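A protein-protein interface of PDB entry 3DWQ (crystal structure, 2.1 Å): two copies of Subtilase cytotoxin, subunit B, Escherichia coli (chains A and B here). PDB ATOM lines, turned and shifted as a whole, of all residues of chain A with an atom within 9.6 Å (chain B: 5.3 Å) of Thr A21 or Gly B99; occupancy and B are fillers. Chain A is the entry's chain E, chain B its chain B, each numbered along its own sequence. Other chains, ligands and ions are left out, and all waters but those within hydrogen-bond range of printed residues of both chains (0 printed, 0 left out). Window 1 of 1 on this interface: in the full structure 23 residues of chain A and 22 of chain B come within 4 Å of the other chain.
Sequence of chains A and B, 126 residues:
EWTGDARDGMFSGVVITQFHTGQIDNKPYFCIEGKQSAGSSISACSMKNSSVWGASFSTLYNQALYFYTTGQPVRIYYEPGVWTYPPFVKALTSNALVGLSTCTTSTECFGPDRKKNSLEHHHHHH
CA of Ser B101 touches O of Phe A19, 3.4 Å away. His A20 touches Tyr B77 (CE1 to CE2, 3.7 Å). Thr A21 touches Thr B59 (OG1 to CG2, 3.1 Å). CG2 of Thr A21 touches CG of Gln B63, at 3.98 Å. Gly B99 touches Thr A21 (CA to O, 3.2 Å). Thr B3 touches Gly A22 (OG1 to CA, 3.2 Å). O of Val B98 touches N of Gln A23, at 3.9 Å. Thr B59 touches Pro A28 (OG1 to CB, 3.9 Å). CB of Thr B3 touches OH of Tyr A29, at 3.9 Å. Thr B59 touches Tyr A61.
Of the printed residues of chain B, Phe A19 touches Gln B63 (3.5 Å) and Ser B101 (3.4 Å). Of the printed residues of chain B, Thr A21 touches Thr B59, Leu B60, Gln B63, Gly B99 and Leu B100. Printed residues of chain B within 4 Å of Gly A22: Thr B3 and Val B98. Printed residues of chain B within 4 Å of Leu A65: Gln B63. Of the printed residues of chain A, Val B98 touches Gly A22 (3.7 Å) and Gln A23 (3.9 Å). Gly B99 touches just one residue of chain A: Thr A21. Of chain A, only His A20 and Thr A21 come within 4 Å of Leu B100. The nearest printed residue of chain B that does not touch Thr A21 is Val B98 (4.7 Å). The nearest printed residue of chain B that does not touch Gln A23 is Gly B99 (5.7 Å).
No position is printed for both chains. Of the 20 pairs that touch across the chains among the printed residues, none has its exchanged pair printed and touching as well.
The side-chain hydroxyl (OG1) of Thr B3 sits at hydrogen-bond distance from the backbone NH (N) of Gln A23, 2.8 Å away. The side-chain hydroxyl of Tyr A61 lies within hydrogen-bond range of the side-chain amide nitrogen of Gln B63 (2.7 Å). The backbone carbonyl oxygen (O) of Leu B100 lies within hydrogen-bond range of a ring nitrogen (ND1) of His A20. N of Thr A21 is in hydrogen-bond range of O of Leu B100. ND1 of His A20 is in hydrogen-bond range of OG of Ser B101 (2.7 Å).
The side-chain hydroxyl (OG1) of Thr B3 sits at hydrogen-bond distance from the backbone carbonyl oxygen (O) of Val B98. O of Tyr B77 sits at hydrogen-bond distance from N of Val B98 (2.9 Å). The backbone NH of Tyr B77 is in hydrogen-bond range of the backbone carbonyl oxygen of Gly B99. O of Tyr A29 is in hydrogen-bond range of OG1 of Thr A21 (2.8 Å). N of Gly A22 is in hydrogen-bond range of O of Tyr A29. O of Pro A28 lies within hydrogen-bond range of N of Lys A48 (2.9 Å).
Of the 12 printed residues of chain B, 9 touch a printed residue of chain A. Hydrophobic or aromatic side chains of chain B within 4 Å of the printed part of chain A: Leu B60 and Tyr B77. Along chain A the printed residues that touch a printed residue of chain B span positions 19 to 65.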
ATOM      1  N   GLN A  18      -6.718 -17.609  39.220  1.00  0.00           N
ATOM      2  CA  GLN A  18      -6.617 -18.968  38.691  1.00  0.00           C
ATOM      3  C   GLN A  18      -6.409 -18.964  37.178  1.00  0.00           C
ATOM      4  O   GLN A  18      -6.916 -18.091  36.471  1.00  0.00           O
ATOM      5  CB  GLN A  18      -7.853 -19.806  39.050  1.00  0.00           C
ATOM      6  CG  GLN A  18      -8.171 -19.952  40.554  1.00  0.00           C
ATOM      7  CD  GLN A  18      -7.118 -20.726  41.350  1.00  0.00           C
ATOM      8  OE1 GLN A  18      -6.533 -21.711  40.873  1.00  0.00           O
ATOM      9  NE2 GLN A  18      -6.881 -20.281  42.580  1.00  0.00           N
ATOM     10  N   PHE A  19      -5.659 -19.953  36.700  1.00  0.00           N
ATOM     11  CA  PHE A  19      -5.312 -20.068  35.288  1.00  0.00           C
ATOM     12  C   PHE A  19      -5.400 -21.533  34.858  1.00  0.00           C
ATOM     13  O   PHE A  19      -4.835 -22.423  35.502  1.00  0.00           O
ATOM     14  CB  PHE A  19      -3.898 -19.528  35.051  1.00  0.00           C
ATOM     15  CG  PHE A  19      -3.694 -18.907  33.693  1.00  0.00           C
ATOM     16  CD1 PHE A  19      -3.593 -17.525  33.560  1.00  0.00           C
ATOM     17  CD2 PHE A  19      -3.595 -19.702  32.552  1.00  0.00           C
ATOM     18  CE1 PHE A  19      -3.395 -16.940  32.310  1.00  0.00           C
ATOM     19  CE2 PHE A  19      -3.399 -19.127  31.294  1.00  0.00           C
ATOM     20  CZ  PHE A  19      -3.298 -17.742  31.173  1.00  0.00           C
ATOM     21  N   HIS A  20      -6.129 -21.773  33.776  1.00  0.00           N
ATOM     22  CA  HIS A  20      -6.257 -23.106  33.204  1.00  0.00           C
ATOM     23  C   HIS A  20      -6.047 -23.045  31.701  1.00  0.00           C
ATOM     24  O   HIS A  20      -6.522 -22.124  31.039  1.00  0.00           O
ATOM     25  CB  HIS A  20      -7.634 -23.702  33.524  1.00  0.00           C
ATOM     26  CG  HIS A  20      -8.008 -24.873  32.667  1.00  0.00           C
ATOM     27  ND1 HIS A  20      -7.381 -26.097  32.761  1.00  0.00           N
ATOM     28  CD2 HIS A  20      -8.958 -25.012  31.712  1.00  0.00           C
ATOM     29  CE1 HIS A  20      -7.921 -26.936  31.895  1.00  0.00           C
ATOM     30  NE2 HIS A  20      -8.881 -26.302  31.246  1.00  0.00           N
ATOM     31  N   THR A  21      -5.329 -24.027  31.169  1.00  0.00           N
ATOM     32  CA  THR A  21      -5.173 -24.156  29.727  1.00  0.00           C
ATOM     33  C   THR A  21      -5.404 -25.597  29.271  1.00  0.00           C
ATOM     34  O   THR A  21      -5.082 -26.548  29.987  1.00  0.00           O
ATOM     35  CB  THR A  21      -3.808 -23.594  29.231  1.00  0.00           C
ATOM     36  OG1 THR A  21      -3.884 -23.338  27.825  1.00  0.00           O
ATOM     37  CG2 THR A  21      -2.653 -24.556  29.521  1.00  0.00           C
ATOM     38  N   GLY A  22      -5.991 -25.747  28.091  1.00  0.00           N
ATOM     39  CA  GLY A  22      -6.281 -27.069  27.548  1.00  0.00           C
ATOM     40  C   GLY A  22      -6.536 -27.042  26.057  1.00  0.00           C
ATOM     41  O   GLY A  22      -6.103 -26.124  25.362  1.00  0.00           O
ATOM     42  N   GLN A  23      -7.244 -28.060  25.574  1.00  0.00           N
ATOM     43  CA  GLN A  23      -7.591 -28.182  24.160  1.00  0.00           C
ATOM     44  C   GLN A  23      -8.962 -28.821  24.012  1.00  0.00           C
ATOM     45  O   GLN A  23      -9.311 -29.734  24.761  1.00  0.00           O
ATOM     46  CB  GLN A  23      -6.550 -29.027  23.420  1.00  0.00           C
ATOM     47  CG  GLN A  23      -6.742 -29.091  21.905  1.00  0.00           C
ATOM     48  CD  GLN A  23      -5.754 -30.015  21.227  1.00  0.00           C
ATOM     49  OE1 GLN A  23      -4.545 -29.834  21.330  1.00  0.00           O
ATOM     50  NE2 GLN A  23      -6.269 -31.017  20.525  1.00  0.00           N
ATOM     51  N   ILE A  24      -9.733 -28.327  23.049  1.00  0.00           N
ATOM     52  CA  ILE A  24     -11.009 -28.936  22.674  1.00  0.00           C
ATOM     53  C   ILE A  24     -11.232 -28.795  21.168  1.00  0.00           C
ATOM     54  O   ILE A  24     -11.035 -27.713  20.603  1.00  0.00           O
ATOM     55  CB  ILE A  24     -12.204 -28.354  23.495  1.00  0.00           C
ATOM     56  CG1 ILE A  24     -13.526 -29.049  23.122  1.00  0.00           C
ATOM     57  CG2 ILE A  24     -12.283 -26.826  23.354  1.00  0.00           C
ATOM     58  CD1 ILE A  24     -14.623 -28.908  24.165  1.00  0.00           C
ATOM     59  N   LYS A  27      -8.499 -27.281  19.105  1.00  0.00           N
ATOM     60  CA  LYS A  27      -8.271 -25.859  19.367  1.00  0.00           C
ATOM     61  C   LYS A  27      -7.747 -25.648  20.786  1.00  0.00           C
ATOM     62  O   LYS A  27      -8.385 -26.075  21.747  1.00  0.00           O
ATOM     63  CB  LYS A  27      -9.566 -25.058  19.182  1.00  0.00           C
ATOM     64  CG  LYS A  27     -10.125 -25.070  17.764  1.00  0.00           C
ATOM     65  CD  LYS A  27     -11.450 -24.322  17.685  1.00  0.00           C
ATOM     66  CE  LYS A  27     -12.094 -24.482  16.313  1.00  0.00           C
ATOM     67  NZ  LYS A  27     -11.210 -23.996  15.207  1.00  0.00           N
ATOM     68  N   PRO A  28      -6.586 -24.983  20.921  1.00  0.00           N
ATOM     69  CA  PRO A  28      -6.107 -24.624  22.256  1.00  0.00           C
ATOM     70  C   PRO A  28      -6.963 -23.522  22.885  1.00  0.00           C
ATOM     71  O   PRO A  28      -7.480 -22.656  22.177  1.00  0.00           O
ATOM     72  CB  PRO A  28      -4.687 -24.117  21.997  1.00  0.00           C
ATOM     73  CG  PRO A  28      -4.697 -23.655  20.587  1.00  0.00           C
ATOM     74  CD  PRO A  28      -5.661 -24.541  19.861  1.00  0.00           C
ATOM     75  N   TYR A  29      -7.113 -23.574  24.205  1.00  0.00           N
ATOM     76  CA  TYR A  29      -7.883 -22.569  24.929  1.00  0.00           C
ATOM     77  C   TYR A  29      -7.276 -22.318  26.301  1.00  0.00           C
ATOM     78  O   TYR A  29      -6.512 -23.135  26.815  1.00  0.00           O
ATOM     79  CB  TYR A  29      -9.361 -22.984  25.066  1.00  0.00           C
ATOM     80  CG  TYR A  29      -9.609 -24.090  26.076  1.00  0.00           C
ATOM     81  CD1 TYR A  29      -9.841 -23.798  27.423  1.00  0.00           C
ATOM     82  CD2 TYR A  29      -9.612 -25.425  25.684  1.00  0.00           C
ATOM     83  CE1 TYR A  29     -10.061 -24.809  28.353  1.00  0.00           C
ATOM     84  CE2 TYR A  29      -9.837 -26.444  26.609  1.00  0.00           C
ATOM     85  CZ  TYR A  29     -10.055 -26.131  27.935  1.00  0.00           C
ATOM     86  OH  TYR A  29     -10.272 -27.143  28.840  1.00  0.00           O
ATOM     87  N   PHE A  30      -7.619 -21.178  26.887  1.00  0.00           N
ATOM     88  CA  PHE A  30      -7.268 -20.902  28.268  1.00  0.00           C
ATOM     89  C   PHE A  30      -8.440 -20.226  28.962  1.00  0.00           C
ATOM     90  O   PHE A  30      -9.233 -19.528  28.323  1.00  0.00           O
ATOM     91  CB  PHE A  30      -5.987 -20.058  28.368  1.00  0.00           C
ATOM     92  CG  PHE A  30      -6.196 -18.585  28.113  1.00  0.00           C
ATOM     93  CD1 PHE A  30      -6.429 -17.708  29.173  1.00  0.00           C
ATOM     94  CD2 PHE A  30      -6.148 -18.075  26.818  1.00  0.00           C
ATOM     95  CE1 PHE A  30      -6.619 -16.341  28.944  1.00  0.00           C
ATOM     96  CE2 PHE A  30      -6.335 -16.715  26.577  1.00  0.00           C
ATOM     97  CZ  PHE A  30      -6.573 -15.845  27.642  1.00  0.00           C
ATOM     98  N   CYS A  31      -8.553 -20.454  30.266  1.00  0.00           N
ATOM     99  CA  CYS A  31      -9.560 -19.790  31.083  1.00  0.00           C
ATOM    100  C   CYS A  31      -8.907 -19.133  32.284  1.00  0.00           C
ATOM    101  O   CYS A  31      -7.907 -19.629  32.811  1.00  0.00           O
ATOM    102  CB  CYS A  31     -10.627 -20.778  31.554  1.00  0.00           C
ATOM    103  SG  CYS A  31     -11.395 -21.730  30.236  1.00  0.00           S
ATOM    104  N   ILE A  32      -9.475 -18.008  32.703  1.00  0.00           N
ATOM    105  CA  ILE A  32      -9.031 -17.331  33.915  1.00  0.00           C
ATOM    106  C   ILE A  32     -10.190 -17.161  34.890  1.00  0.00           C
ATOM    107  O   ILE A  32     -11.348 -17.065  34.485  1.00  0.00           O
ATOM    108  CB  ILE A  32      -8.356 -15.960  33.619  1.00  0.00           C
ATOM    109  CG1 ILE A  32      -9.251 -15.085  32.726  1.00  0.00           C
ATOM    110  CG2 ILE A  32      -6.974 -16.175  32.996  1.00  0.00           C
ATOM    111  CD1 ILE A  32      -8.789 -13.644  32.585  1.00  0.00           C
ATOM    112  N   ALA A  44     -13.797 -16.469  32.565  1.00  0.00           N
ATOM    113  CA  ALA A  44     -13.858 -16.253  31.119  1.00  0.00           C
ATOM    114  C   ALA A  44     -12.801 -17.083  30.399  1.00  0.00           C
ATOM    115  O   ALA A  44     -11.681 -17.239  30.896  1.00  0.00           O
ATOM    116  CB  ALA A  44     -13.702 -14.767  30.788  1.00  0.00           C
ATOM    117  N   CYS A  45     -13.162 -17.609  29.231  1.00  0.00           N
ATOM    118  CA  CYS A  45     -12.244 -18.409  28.421  1.00  0.00           C
ATOM    119  C   CYS A  45     -11.995 -17.801  27.038  1.00  0.00           C
ATOM    120  O   CYS A  45     -12.892 -17.207  26.433  1.00  0.00           O
ATOM    121  CB  CYS A  45     -12.756 -19.847  28.266  1.00  0.00           C
ATOM    122  SG  CYS A  45     -13.113 -20.717  29.813  1.00  0.00           S
ATOM    123  N   SER A  46     -10.771 -17.962  26.546  1.00  0.00           N
ATOM    124  CA  SER A  46     -10.434 -17.591  25.178  1.00  0.00           C
ATOM    125  C   SER A  46      -9.949 -18.826  24.419  1.00  0.00           C
ATOM    126  O   SER A  46      -9.090 -19.563  24.908  1.00  0.00           O
ATOM    127  CB  SER A  46      -9.378 -16.484  25.159  1.00  0.00           C
ATOM    128  OG  SER A  46      -8.989 -16.169  23.833  1.00  0.00           O
ATOM    129  N   MET A  47     -10.516 -19.048  23.236  1.00  0.00           N
ATOM    130  CA  MET A  47     -10.226 -20.236  22.436  1.00  0.00           C
ATOM    131  C   MET A  47      -9.745 -19.849  21.041  1.00  0.00           C
ATOM    132  O   MET A  47     -10.410 -19.085  20.339  1.00  0.00           O
ATOM    133  CB  MET A  47     -11.473 -21.118  22.337  1.00  0.00           C
ATOM    134  CG  MET A  47     -11.249 -22.500  21.728  1.00  0.00           C
ATOM    135  SD  MET A  47     -12.795 -23.420  21.522  1.00  0.00           S
ATOM    136  CE  MET A  47     -13.420 -23.456  23.204  1.00  0.00           C
ATOM    137  N   LYS A  48      -8.594 -20.391  20.652  1.00  0.00           N
ATOM    138  CA  LYS A  48      -7.988 -20.098  19.353  1.00  0.00           C
ATOM    139  C   LYS A  48      -8.850 -20.606  18.199  1.00  0.00           C
ATOM    140  O   LYS A  48      -9.381 -21.719  18.248  1.00  0.00           O
ATOM    141  CB  LYS A  48      -6.585 -20.705  19.273  1.00  0.00           C
ATOM    142  CG  LYS A  48      -5.727 -20.197  18.124  1.00  0.00           C
ATOM    143  CD  LYS A  48      -4.457 -21.025  17.997  1.00  0.00           C
ATOM    144  CE  LYS A  48      -3.530 -20.482  16.923  1.00  0.00           C
ATOM    145  NZ  LYS A  48      -2.288 -21.300  16.837  1.00  0.00           N
ATOM    146  N   PHE A  57      -6.900 -14.649  20.712  1.00  0.00           N
ATOM    147  CA  PHE A  57      -6.463 -15.699  21.645  1.00  0.00           C
ATOM    148  C   PHE A  57      -5.052 -15.500  22.206  1.00  0.00           C
ATOM    149  O   PHE A  57      -4.869 -15.509  23.425  1.00  0.00           O
ATOM    150  CB  PHE A  57      -6.592 -17.101  21.021  1.00  0.00           C
ATOM    151  CG  PHE A  57      -5.868 -18.182  21.795  1.00  0.00           C
ATOM    152  CD1 PHE A  57      -6.443 -18.751  22.925  1.00  0.00           C
ATOM    153  CD2 PHE A  57      -4.607 -18.627  21.391  1.00  0.00           C
ATOM    154  CE1 PHE A  57      -5.778 -19.746  23.646  1.00  0.00           C
ATOM    155  CE2 PHE A  57      -3.935 -19.622  22.103  1.00  0.00           C
ATOM    156  CZ  PHE A  57      -4.523 -20.184  23.232  1.00  0.00           C
ATOM    157  N   TYR A  61      -3.912 -14.352  25.847  1.00  0.00           N
ATOM    158  CA  TYR A  61      -3.145 -15.332  26.614  1.00  0.00           C
ATOM    159  C   TYR A  61      -1.936 -14.669  27.256  1.00  0.00           C
ATOM    160  O   TYR A  61      -1.708 -14.824  28.456  1.00  0.00           O
ATOM    161  CB  TYR A  61      -2.706 -16.530  25.758  1.00  0.00           C
ATOM    162  CG  TYR A  61      -1.715 -17.429  26.476  1.00  0.00           C
ATOM    163  CD1 TYR A  61      -2.146 -18.370  27.411  1.00  0.00           C
ATOM    164  CD2 TYR A  61      -0.342 -17.314  26.243  1.00  0.00           C
ATOM    165  CE1 TYR A  61      -1.239 -19.183  28.085  1.00  0.00           C
ATOM    166  CE2 TYR A  61       0.575 -18.119  26.913  1.00  0.00           C
ATOM    167  CZ  TYR A  61       0.120 -19.053  27.831  1.00  0.00           C
ATOM    168  OH  TYR A  61       1.027 -19.854  28.494  1.00  0.00           O
ATOM    169  N   LEU A  65      -1.760 -13.831  31.352  1.00  0.00           N
ATOM    170  CA  LEU A  65      -0.665 -14.441  32.099  1.00  0.00           C
ATOM    171  C   LEU A  65       0.242 -13.367  32.696  1.00  0.00           C
ATOM    172  O   LEU A  65       0.761 -13.540  33.801  1.00  0.00           O
ATOM    173  CB  LEU A  65       0.133 -15.426  31.231  1.00  0.00           C
ATOM    174  CG  LEU A  65       1.229 -16.257  31.920  1.00  0.00           C
ATOM    175  CD1 LEU A  65       0.650 -17.217  32.955  1.00  0.00           C
ATOM    176  CD2 LEU A  65       2.068 -17.011  30.890  1.00  0.00           C
ATOM    177  N   PHE A  88     -18.224 -28.482  29.092  1.00  0.00           N
ATOM    178  CA  PHE A  88     -17.297 -27.349  29.123  1.00  0.00           C
ATOM    179  C   PHE A  88     -17.866 -26.198  29.952  1.00  0.00           C
ATOM    180  O   PHE A  88     -17.169 -25.627  30.789  1.00  0.00           O
ATOM    181  CB  PHE A  88     -16.981 -26.878  27.696  1.00  0.00           C
ATOM    182  CG  PHE A  88     -15.882 -25.851  27.611  1.00  0.00           C
ATOM    183  CD1 PHE A  88     -14.583 -26.230  27.288  1.00  0.00           C
ATOM    184  CD2 PHE A  88     -16.149 -24.500  27.833  1.00  0.00           C
ATOM    185  CE1 PHE A  88     -13.562 -25.280  27.197  1.00  0.00           C
ATOM    186  CE2 PHE A  88     -15.134 -23.542  27.749  1.00  0.00           C
ATOM    187  CZ  PHE A  88     -13.843 -23.933  27.428  1.00  0.00           C
ATOM    188  N   LEU A  92     -16.306 -25.129  33.437  1.00  0.00           N
ATOM    189  CA  LEU A  92     -15.665 -23.819  33.336  1.00  0.00           C
ATOM    190  C   LEU A  92     -16.677 -22.670  33.263  1.00  0.00           C
ATOM    191  O   LEU A  92     -17.089 -22.140  34.297  1.00  0.00           O
ATOM    192  CB  LEU A  92     -14.688 -23.790  32.150  1.00  0.00           C
ATOM    193  CG  LEU A  92     -13.442 -24.686  32.220  1.00  0.00           C
ATOM    194  CD1 LEU A  92     -12.983 -25.091  30.830  1.00  0.00           C
ATOM    195  CD2 LEU A  92     -12.305 -24.018  32.983  1.00  0.00           C
ATOM    196  N   THR B   3      -9.670 -31.763  26.906  1.00  0.00           N
ATOM    197  CA  THR B   3      -8.925 -31.873  28.155  1.00  0.00           C
ATOM    198  C   THR B   3      -9.777 -32.436  29.309  1.00  0.00           C
ATOM    199  O   THR B   3      -9.310 -33.284  30.076  1.00  0.00           O
ATOM    200  CB  THR B   3      -8.323 -30.493  28.530  1.00  0.00           C
ATOM    201  OG1 THR B   3      -7.442 -30.068  27.484  1.00  0.00           O
ATOM    202  CG2 THR B   3      -7.546 -30.552  29.828  1.00  0.00           C
ATOM    203  N   THR B  59       1.116 -23.358  23.511  1.00  0.00           N
ATOM    204  CA  THR B  59       0.498 -22.886  24.754  1.00  0.00           C
ATOM    205  C   THR B  59       1.033 -23.646  25.970  1.00  0.00           C
ATOM    206  O   THR B  59       1.405 -23.035  26.977  1.00  0.00           O
ATOM    207  CB  THR B  59      -1.048 -22.991  24.702  1.00  0.00           C
ATOM    208  OG1 THR B  59      -1.534 -22.378  23.503  1.00  0.00           O
ATOM    209  CG2 THR B  59      -1.686 -22.300  25.906  1.00  0.00           C
ATOM    210  N   LEU B  60       1.079 -24.973  25.862  1.00  0.00           N
ATOM    211  CA  LEU B  60       1.546 -25.825  26.954  1.00  0.00           C
ATOM    212  C   LEU B  60       3.035 -25.660  27.254  1.00  0.00           C
ATOM    213  O   LEU B  60       3.434 -25.736  28.417  1.00  0.00           O
ATOM    214  CB  LEU B  60       1.203 -27.300  26.698  1.00  0.00           C
ATOM    215  CG  LEU B  60      -0.281 -27.687  26.759  1.00  0.00           C
ATOM    216  CD1 LEU B  60      -0.495 -29.092  26.218  1.00  0.00           C
ATOM    217  CD2 LEU B  60      -0.839 -27.560  28.170  1.00  0.00           C
ATOM    218  N   GLN B  63       3.255 -22.358  29.211  1.00  0.00           N
ATOM    219  CA  GLN B  63       2.640 -22.536  30.522  1.00  0.00           C
ATOM    220  C   GLN B  63       3.464 -23.455  31.428  1.00  0.00           C
ATOM    221  O   GLN B  63       3.649 -23.155  32.607  1.00  0.00           O
ATOM    222  CB  GLN B  63       1.200 -23.047  30.363  1.00  0.00           C
ATOM    223  CG  GLN B  63       0.264 -22.735  31.534  1.00  0.00           C
ATOM    224  CD  GLN B  63       0.159 -21.252  31.860  1.00  0.00           C
ATOM    225  OE1 GLN B  63       0.387 -20.842  32.997  1.00  0.00           O
ATOM    226  NE2 GLN B  63      -0.183 -20.444  30.868  1.00  0.00           N
ATOM    227  N   ARG B  75      -1.948 -28.664  38.266  1.00  0.00           N
ATOM    228  CA  ARG B  75      -2.561 -29.887  37.760  1.00  0.00           C
ATOM    229  C   ARG B  75      -2.016 -30.237  36.378  1.00  0.00           C
ATOM    230  O   ARG B  75      -1.944 -29.382  35.494  1.00  0.00           O
ATOM    231  CB  ARG B  75      -4.089 -29.769  37.718  1.00  0.00           C
ATOM    232  CG  ARG B  75      -4.794 -31.019  37.187  1.00  0.00           C
ATOM    233  CD  ARG B  75      -6.304 -30.894  37.261  1.00  0.00           C
ATOM    234  NE  ARG B  75      -6.811 -31.059  38.621  1.00  0.00           N
ATOM    235  CZ  ARG B  75      -8.056 -30.785  38.999  1.00  0.00           C
ATOM    236  NH1 ARG B  75      -8.942 -30.325  38.125  1.00  0.00           N
ATOM    237  NH2 ARG B  75      -8.415 -30.974  40.261  1.00  0.00           N
ATOM    238  N   ILE B  76      -1.623 -31.497  36.211  1.00  0.00           N
ATOM    239  CA  ILE B  76      -1.221 -32.020  34.912  1.00  0.00           C
ATOM    240  C   ILE B  76      -2.338 -32.905  34.371  1.00  0.00           C
ATOM    241  O   ILE B  76      -2.702 -33.912  34.986  1.00  0.00           O
ATOM    242  CB  ILE B  76       0.123 -32.812  34.979  1.00  0.00           C
ATOM    243  CG1 ILE B  76       1.315 -31.860  35.043  1.00  0.00           C
ATOM    244  CG2 ILE B  76       0.304 -33.715  33.765  1.00  0.00           C
ATOM    245  CD1 ILE B  76       1.687 -31.427  36.424  1.00  0.00           C
ATOM    246  N   TYR B  77      -2.893 -32.495  33.236  1.00  0.00           N
ATOM    247  CA  TYR B  77      -3.846 -33.302  32.492  1.00  0.00           C
ATOM    248  C   TYR B  77      -3.057 -34.088  31.459  1.00  0.00           C
ATOM    249  O   TYR B  77      -2.246 -33.517  30.722  1.00  0.00           O
ATOM    250  CB  TYR B  77      -4.867 -32.420  31.771  1.00  0.00           C
ATOM    251  CG  TYR B  77      -5.783 -31.587  32.645  1.00  0.00           C
ATOM    252  CD1 TYR B  77      -7.049 -32.054  33.006  1.00  0.00           C
ATOM    253  CD2 TYR B  77      -5.404 -30.314  33.072  1.00  0.00           C
ATOM    254  CE1 TYR B  77      -7.907 -31.278  33.788  1.00  0.00           C
ATOM    255  CE2 TYR B  77      -6.247 -29.536  33.854  1.00  0.00           C
ATOM    256  CZ  TYR B  77      -7.498 -30.022  34.207  1.00  0.00           C
ATOM    257  OH  TYR B  77      -8.332 -29.248  34.980  1.00  0.00           O
ATOM    258  N   LEU B  97       0.813 -34.501  27.249  1.00  0.00           N
ATOM    259  CA  LEU B  97       0.326 -33.388  28.057  1.00  0.00           C
ATOM    260  C   LEU B  97      -0.837 -32.740  27.312  1.00  0.00           C
ATOM    261  O   LEU B  97      -0.688 -32.310  26.163  1.00  0.00           O
ATOM    262  CB  LEU B  97       1.449 -32.379  28.337  1.00  0.00           C
ATOM    263  CG  LEU B  97       1.152 -31.200  29.276  1.00  0.00           C
ATOM    264  CD1 LEU B  97       0.787 -31.660  30.686  1.00  0.00           C
ATOM    265  CD2 LEU B  97       2.338 -30.242  29.318  1.00  0.00           C
ATOM    266  N   VAL B  98      -2.000 -32.704  27.959  1.00  0.00           N
ATOM    267  CA  VAL B  98      -3.229 -32.248  27.305  1.00  0.00           C
ATOM    268  C   VAL B  98      -3.848 -31.017  27.984  1.00  0.00           C
ATOM    269  O   VAL B  98      -4.864 -30.489  27.528  1.00  0.00           O
ATOM    270  CB  VAL B  98      -4.274 -33.406  27.138  1.00  0.00           C
ATOM    271  CG1 VAL B  98      -3.608 -34.651  26.576  1.00  0.00           C
ATOM    272  CG2 VAL B  98      -4.980 -33.736  28.453  1.00  0.00           C
ATOM    273  N   GLY B  99      -3.223 -30.565  29.066  1.00  0.00           N
ATOM    274  CA  GLY B  99      -3.696 -29.391  29.792  1.00  0.00           C
ATOM    275  C   GLY B  99      -2.958 -29.124  31.089  1.00  0.00           C
ATOM    276  O   GLY B  99      -2.263 -29.998  31.608  1.00  0.00           O
ATOM    277  N   LEU B 100      -3.126 -27.907  31.607  1.00  0.00           N
ATOM    278  CA  LEU B 100      -2.513 -27.473  32.862  1.00  0.00           C
ATOM    279  C   LEU B 100      -3.453 -26.549  33.636  1.00  0.00           C
ATOM    280  O   LEU B 100      -4.200 -25.772  33.038  1.00  0.00           O
ATOM    281  CB  LEU B 100      -1.187 -26.745  32.597  1.00  0.00           C
ATOM    282  CG  LEU B 100       0.030 -27.556  32.135  1.00  0.00           C
ATOM    283  CD1 LEU B 100       1.107 -26.651  31.534  1.00  0.00           C
ATOM    284  CD2 LEU B 100       0.601 -28.408  33.271  1.00  0.00           C
ATOM    285  N   SER B 101      -3.407 -26.630  34.963  1.00  0.00           N
ATOM    286  CA  SER B 101      -4.220 -25.763  35.818  1.00  0.00           C
ATOM    287  C   SER B 101      -3.474 -25.313  37.065  1.00  0.00           C
ATOM    288  O   SER B 101      -2.661 -26.058  37.600  1.00  0.00           O
ATOM    289  CB  SER B 101      -5.497 -26.483  36.250  1.00  0.00           C
ATOM    290  OG  SER B 101      -6.454 -26.512  35.212  1.00  0.00           O
